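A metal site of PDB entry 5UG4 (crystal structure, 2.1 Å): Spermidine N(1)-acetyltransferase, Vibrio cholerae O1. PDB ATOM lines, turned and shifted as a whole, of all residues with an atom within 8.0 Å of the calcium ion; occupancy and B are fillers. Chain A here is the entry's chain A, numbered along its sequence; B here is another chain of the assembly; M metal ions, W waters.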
ATOM      1  N   MET A  28     -23.238  23.206   1.776  1.00  0.00           N
ATOM      2  CA  MET A  28     -23.146  22.893   3.210  1.00  0.00           C
ATOM      3  C   MET A  28     -21.671  22.851   3.642  1.00  0.00           C
ATOM      4  O   MET A  28     -20.865  22.142   3.041  1.00  0.00           O
ATOM      5  CB  MET A  28     -23.797  21.565   3.577  1.00  0.00           C
ATOM      6  CG  MET A  28     -23.800  21.275   5.083  1.00  0.00           C
ATOM      7  SD  MET A  28     -24.708  22.489   6.083  1.00  0.00           S
ATOM      8  CE  MET A  28     -26.346  22.124   5.578  1.00  0.00           C
ATOM      9  N   SER A  29     -21.353  23.628   4.649  1.00  0.00           N
ATOM     10  CA  SER A  29     -20.010  23.677   5.210  1.00  0.00           C
ATOM     11  C   SER A  29     -19.924  22.879   6.532  1.00  0.00           C
ATOM     12  O   SER A  29     -20.943  22.638   7.192  1.00  0.00           O
ATOM     13  CB  SER A  29     -19.605  25.128   5.461  1.00  0.00           C
ATOM     14  OG  SER A  29     -19.650  25.814   4.226  1.00  0.00           O
ATOM     15  N   GLU A  33     -16.273  17.883  10.923  1.00  0.00           N
ATOM     16  CA  GLU A  33     -17.347  16.985  10.479  1.00  0.00           C
ATOM     17  C   GLU A  33     -18.726  17.413  10.921  1.00  0.00           C
ATOM     18  O   GLU A  33     -19.671  16.743  10.571  1.00  0.00           O
ATOM     19  CB  GLU A  33     -17.138  15.498  10.915  1.00  0.00           C
ATOM     20  CG  GLU A  33     -15.729  14.973  10.812  1.00  0.00           C
ATOM     21  CD  GLU A  33     -15.447  14.245   9.526  1.00  0.00           C
ATOM     22  OE1 GLU A  33     -16.229  14.432   8.535  1.00  0.00           O
ATOM     23  OE2 GLU A  33     -14.444  13.480   9.479  1.00  0.00           O
ATOM     24  N   GLU A  34     -18.884  18.497  11.696  1.00  0.00           N
ATOM     25  CA  GLU A  34     -20.206  18.980  12.077  1.00  0.00           C
ATOM     26  C   GLU A  34     -20.650  19.962  10.967  1.00  0.00           C
ATOM     27  O   GLU A  34     -19.949  20.938  10.684  1.00  0.00           O
ATOM     28  CB  GLU A  34     -20.203  19.633  13.471  1.00  0.00           C
ATOM     29  CG  GLU A  34     -21.534  20.422  13.793  1.00  0.00           C
ATOM     30  CD  GLU A  34     -22.804  19.564  13.898  1.00  0.00           C
ATOM     31  OE1 GLU A  34     -22.646  18.374  14.309  1.00  0.00           O
ATOM     32  OE2 GLU A  34     -23.938  20.098  13.611  1.00  0.00           O
ATOM     33  N   PRO A  35     -21.819  19.728  10.358  1.00  0.00           N
ATOM     34  CA  PRO A  35     -22.362  20.712   9.436  1.00  0.00           C
ATOM     35  C   PRO A  35     -22.798  21.947  10.156  1.00  0.00           C
ATOM     36  O   PRO A  35     -23.260  21.856  11.296  1.00  0.00           O
ATOM     37  CB  PRO A  35     -23.598  19.971   8.820  1.00  0.00           C
ATOM     38  CG  PRO A  35     -24.053  19.015   9.905  1.00  0.00           C
ATOM     39  CD  PRO A  35     -22.713  18.538  10.510  1.00  0.00           C
ATOM     40  N   TYR A  36     -22.618  23.115   9.550  1.00  0.00           N
ATOM     41  CA  TYR A  36     -23.102  24.326  10.176  1.00  0.00           C
ATOM     42  C   TYR A  36     -23.526  25.265   9.098  1.00  0.00           C
ATOM     43  O   TYR A  36     -22.971  25.216   7.990  1.00  0.00           O
ATOM     44  CB  TYR A  36     -22.002  24.980  11.028  1.00  0.00           C
ATOM     45  CG  TYR A  36     -20.893  25.569  10.248  1.00  0.00           C
ATOM     46  CD1 TYR A  36     -19.811  24.815   9.864  1.00  0.00           C
ATOM     47  CD2 TYR A  36     -20.960  26.892   9.840  1.00  0.00           C
ATOM     48  CE1 TYR A  36     -18.797  25.355   9.080  1.00  0.00           C
ATOM     49  CE2 TYR A  36     -19.945  27.445   9.068  1.00  0.00           C
ATOM     50  CZ  TYR A  36     -18.884  26.665   8.699  1.00  0.00           C
ATOM     51  OH  TYR A  36     -17.938  27.235   7.940  1.00  0.00           O
ATOM     52  N   GLU A  37     -24.462  26.138   9.443  1.00  0.00           N
ATOM     53  CA  GLU A  37     -24.964  27.214   8.560  1.00  0.00           C
ATOM     54  C   GLU A  37     -24.819  28.614   9.087  1.00  0.00           C
ATOM     55  O   GLU A  37     -24.811  29.555   8.345  1.00  0.00           O
ATOM     56  CB  GLU A  37     -26.460  26.960   8.296  1.00  0.00           C
ATOM     57  CG  GLU A  37     -26.672  25.647   7.580  1.00  0.00           C
ATOM     58  CD  GLU A  37     -27.969  24.961   8.015  1.00  0.00           C
ATOM     59  OE1 GLU A  37     -28.618  25.386   9.006  1.00  0.00           O
ATOM     60  OE2 GLU A  37     -28.318  23.994   7.375  1.00  0.00           O
ATOM     61  N   SER A  38     -24.780  28.768  10.400  1.00  0.00           N
ATOM     62  CA  SER A  38     -24.776  30.122  11.006  1.00  0.00           C
ATOM     63  C   SER A  38     -23.435  30.467  11.547  1.00  0.00           C
ATOM     64  O   SER A  38     -22.662  29.579  11.896  1.00  0.00           O
ATOM     65  CB  SER A  38     -25.769  30.154  12.186  1.00  0.00           C
ATOM     66  OG  SER A  38     -25.406  29.212  13.165  1.00  0.00           O
ATOM     67  N   GLU A  41     -23.087  29.051  15.159  1.00  0.00           N
ATOM     68  CA  GLU A  41     -22.650  27.681  15.325  1.00  0.00           C
ATOM     69  C   GLU A  41     -21.136  27.534  14.910  1.00  0.00           C
ATOM     70  O   GLU A  41     -20.364  26.827  15.585  1.00  0.00           O
ATOM     71  CB  GLU A  41     -23.468  26.626  14.565  1.00  0.00           C
ATOM     72  CG  GLU A  41     -23.035  25.226  15.003  1.00  0.00           C
ATOM     73  CD  GLU A  41     -23.802  24.090  14.372  1.00  0.00           C
ATOM     74  OE1 GLU A  41     -23.653  22.906  14.884  1.00  0.00           O
ATOM     75  OE2 GLU A  41     -24.601  24.336  13.403  1.00  0.00           O
ATOM     76  N   LEU A  42     -20.738  28.282  13.891  1.00  0.00           N
ATOM     77  CA  LEU A  42     -19.322  28.292  13.506  1.00  0.00           C
ATOM     78  C   LEU A  42     -18.439  28.706  14.704  1.00  0.00           C
ATOM     79  O   LEU A  42     -17.471  28.034  15.074  1.00  0.00           O
ATOM     80  CB  LEU A  42     -19.086  29.187  12.317  1.00  0.00           C
ATOM     81  CG  LEU A  42     -17.584  29.370  11.932  1.00  0.00           C
ATOM     82  CD1 LEU A  42     -16.888  28.058  11.578  1.00  0.00           C
ATOM     83  CD2 LEU A  42     -17.552  30.400  10.792  1.00  0.00           C
ATOM     84  N   LEU A  45     -18.309  25.912  17.362  1.00  0.00           N
ATOM     85  CA  LEU A  45     -17.465  24.837  16.907  1.00  0.00           C
ATOM     86  C   LEU A  45     -15.965  25.225  16.937  1.00  0.00           C
ATOM     87  O   LEU A  45     -15.155  24.458  17.355  1.00  0.00           O
ATOM     88  CB  LEU A  45     -17.862  24.392  15.501  1.00  0.00           C
ATOM     89  CG  LEU A  45     -19.209  23.652  15.454  1.00  0.00           C
ATOM     90  CD1 LEU A  45     -19.709  23.598  14.029  1.00  0.00           C
ATOM     91  CD2 LEU A  45     -19.167  22.248  16.060  1.00  0.00           C
ATOM     92  N   HIS B  49     -29.551  24.430  21.993  1.00  0.00           N
ATOM     93  CA  HIS B  49     -29.719  23.498  20.851  1.00  0.00           C
ATOM     94  C   HIS B  49     -28.949  23.878  19.632  1.00  0.00           C
ATOM     95  O   HIS B  49     -29.262  23.463  18.506  1.00  0.00           O
ATOM     96  CB  HIS B  49     -31.266  23.407  20.532  1.00  0.00           C
ATOM     97  CG  HIS B  49     -32.032  22.784  21.618  1.00  0.00           C
ATOM     98  ND1 HIS B  49     -32.161  21.420  21.768  1.00  0.00           N
ATOM     99  CD2 HIS B  49     -32.729  23.336  22.651  1.00  0.00           C
ATOM    100  CE1 HIS B  49     -32.853  21.158  22.857  1.00  0.00           C
ATOM    101  NE2 HIS B  49     -33.244  22.300  23.394  1.00  0.00           N
ATOM    102  N   ILE B  50     -27.939  24.708  19.812  1.00  0.00           N
ATOM    103  CA  ILE B  50     -27.192  25.247  18.720  1.00  0.00           C
ATOM    104  C   ILE B  50     -26.601  24.167  17.789  1.00  0.00           C
ATOM    105  O   ILE B  50     -26.480  24.418  16.617  1.00  0.00           O
ATOM    106  CB  ILE B  50     -26.111  26.254  19.222  1.00  0.00           C
ATOM    107  CG1 ILE B  50     -25.452  27.050  18.111  1.00  0.00           C
ATOM    108  CG2 ILE B  50     -24.941  25.627  19.980  1.00  0.00           C
ATOM    109  CD1 ILE B  50     -26.263  28.266  17.822  1.00  0.00           C
ATOM    110  N   HIS B  51     -26.246  22.999  18.309  1.00  0.00           N
ATOM    111  CA  HIS B  51     -25.612  21.920  17.544  1.00  0.00           C
ATOM    112  C   HIS B  51     -26.615  20.853  17.134  1.00  0.00           C
ATOM    113  O   HIS B  51     -26.248  19.902  16.460  1.00  0.00           O
ATOM    114  CB  HIS B  51     -24.470  21.283  18.335  1.00  0.00           C
ATOM    115  CG  HIS B  51     -23.345  22.225  18.603  1.00  0.00           C
ATOM    116  ND1 HIS B  51     -22.755  22.959  17.600  1.00  0.00           N
ATOM    117  CD2 HIS B  51     -22.763  22.609  19.767  1.00  0.00           C
ATOM    118  CE1 HIS B  51     -21.798  23.710  18.133  1.00  0.00           C
ATOM    119  NE2 HIS B  51     -21.817  23.545  19.446  1.00  0.00           N
ATOM    120  N   ASP B  52     -27.867  21.036  17.489  1.00  0.00           N
ATOM    121  CA  ASP B  52     -28.878  20.092  17.076  1.00  0.00           C
ATOM    122  C   ASP B  52     -29.343  20.324  15.639  1.00  0.00           C
ATOM    123  O   ASP B  52     -29.780  21.433  15.271  1.00  0.00           O
ATOM    124  CB  ASP B  52     -30.025  20.157  18.087  1.00  0.00           C
ATOM    125  CG  ASP B  52     -30.972  18.951  17.982  1.00  0.00           C
ATOM    126  OD1 ASP B  52     -31.179  18.363  16.882  1.00  0.00           O
ATOM    127  OD2 ASP B  52     -31.575  18.677  19.002  1.00  0.00           O
ATOM    128  N   ASN B  53     -29.242  19.296  14.794  1.00  0.00           N
ATOM    129  CA  ASN B  53     -29.569  19.400  13.399  1.00  0.00           C
ATOM    130  C   ASN B  53     -31.037  18.928  13.060  1.00  0.00           C
ATOM    131  O   ASN B  53     -31.423  18.923  11.909  1.00  0.00           O
ATOM    132  CB  ASN B  53     -28.543  18.616  12.549  1.00  0.00           C
ATOM    133  CG  ASN B  53     -27.097  19.203  12.734  1.00  0.00           C
ATOM    134  OD1 ASN B  53     -26.873  20.424  12.646  1.00  0.00           O
ATOM    135  ND2 ASN B  53     -26.148  18.328  13.078  1.00  0.00           N
ATOM    136  N   ALA B  54     -31.827  18.603  14.060  1.00  0.00           N
ATOM    137  CA  ALA B  54     -33.223  18.157  13.865  1.00  0.00           C
ATOM    138  C   ALA B  54     -34.183  19.283  13.491  1.00  0.00           C
ATOM    139  O   ALA B  54     -35.313  19.052  12.975  1.00  0.00           O
ATOM    140  CB  ALA B  54     -33.711  17.420  15.105  1.00  0.00           C
ATOM    141  N   GLU B  55     -33.760  20.535  13.736  1.00  0.00           N
ATOM    142  CA  GLU B  55     -34.501  21.706  13.287  1.00  0.00           C
ATOM    143  C   GLU B  55     -33.538  22.725  12.774  1.00  0.00           C
ATOM    144  O   GLU B  55     -32.479  22.887  13.371  1.00  0.00           O
ATOM    145  CB  GLU B  55     -35.376  22.331  14.413  1.00  0.00           C
ATOM    146  CG  GLU B  55     -36.193  21.303  15.220  1.00  0.00           C
ATOM    147  CD  GLU B  55     -37.074  21.952  16.318  1.00  0.00           C
ATOM    148  OE1 GLU B  55     -37.939  21.208  16.826  1.00  0.00           O
ATOM    149  OE2 GLU B  55     -36.895  23.124  16.736  1.00  0.00           O
ATOM    150  N   ARG B  56     -33.943  23.442  11.725  1.00  0.00           N
ATOM    151  CA  ARG B  56     -33.094  24.439  11.041  1.00  0.00           C
ATOM    152  C   ARG B  56     -33.980  25.606  10.711  1.00  0.00           C
ATOM    153  O   ARG B  56     -35.115  25.390  10.213  1.00  0.00           O
ATOM    154  CB  ARG B  56     -32.513  23.909   9.723  1.00  0.00           C
ATOM    155  CG  ARG B  56     -31.654  22.681   9.821  1.00  0.00           C
ATOM    156  CD  ARG B  56     -30.591  22.677  10.880  1.00  0.00           C
ATOM    157  NE  ARG B  56     -29.642  23.793  10.957  1.00  0.00           N
ATOM    158  CZ  ARG B  56     -29.298  24.426  12.089  1.00  0.00           C
ATOM    159  NH1 ARG B  56     -29.824  24.096  13.297  1.00  0.00           N
ATOM    160  NH2 ARG B  56     -28.371  25.363  12.003  1.00  0.00           N
ATOM    161  N   TYR B  78     -33.036  12.133   9.085  1.00  0.00           N
ATOM    162  CA  TYR B  78     -31.971  11.973   8.097  1.00  0.00           C
ATOM    163  C   TYR B  78     -31.891  10.549   7.549  1.00  0.00           C
ATOM    164  O   TYR B  78     -30.995  10.219   6.791  1.00  0.00           O
ATOM    165  CB  TYR B  78     -30.608  12.504   8.601  1.00  0.00           C
ATOM    166  CG  TYR B  78     -30.553  14.024   8.868  1.00  0.00           C
ATOM    167  CD1 TYR B  78     -30.973  14.563  10.124  1.00  0.00           C
ATOM    168  CD2 TYR B  78     -30.167  14.928   7.888  1.00  0.00           C
ATOM    169  CE1 TYR B  78     -30.962  15.939  10.350  1.00  0.00           C
ATOM    170  CE2 TYR B  78     -30.155  16.307   8.128  1.00  0.00           C
ATOM    171  CZ  TYR B  78     -30.550  16.799   9.366  1.00  0.00           C
ATOM    172  OH  TYR B  78     -30.519  18.169   9.571  1.00  0.00           O
HETATM  173 CA    CA M   1     -25.045  21.995  13.076  1.00  0.00          CA
HETATM  174  O   HOH W   1     -26.996  22.810  14.493  1.00  0.00           O
HETATM  175  O   HOH W   2     -26.255  22.988  11.241  1.00  0.00           O
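Water W1 lies within hydrogen-bond range of O of Ile 50 of chain B (2.7 Å), O of Asp 52 of chain B (3.2 Å) and NH1 of Arg 56 of chain B (3.3 Å).
The side-chain carboxylate (OE2) of Glu 34 is bound to the calcium ion.
OE2 of Glu 41 is bound to the calcium ion (2.4 Å).
The calcium ion is bound by water W2 (2.4 Å).
OD1 of Asn 53 of chain B is bound to the calcium ion (2.4 Å).
The calcium ion is bound by OE1 of Glu 41, at 2.5 Å.
O of Pro 35 is bound to the calcium ion.
Water W1 is bound to the calcium ion, 2.5 Å away.
The calcium ion has seven donor atoms within binding distance.
The side-chain carboxylate (OE1) of Glu 41 lies close to a ring nitrogen (ND1) of His 51 of chain B, at 2.9 Å.
N of Glu 41 is in hydrogen-bond range of OG of Ser 38, 3.1 Å away.
The side-chain hydroxyl (OH) of Tyr 78 of chain B sits at hydrogen-bond distance from the backbone carbonyl oxygen (O) of Asn 53 of chain B, at 2.6 Å.
Within 4 Å of the calcium ion: Glu 34, Pro 35, Glu 41 and Asn 53 of chain B.
The nearest printed residue that does not touch the calcium ion is His 51 of chain B (4.2 Å).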
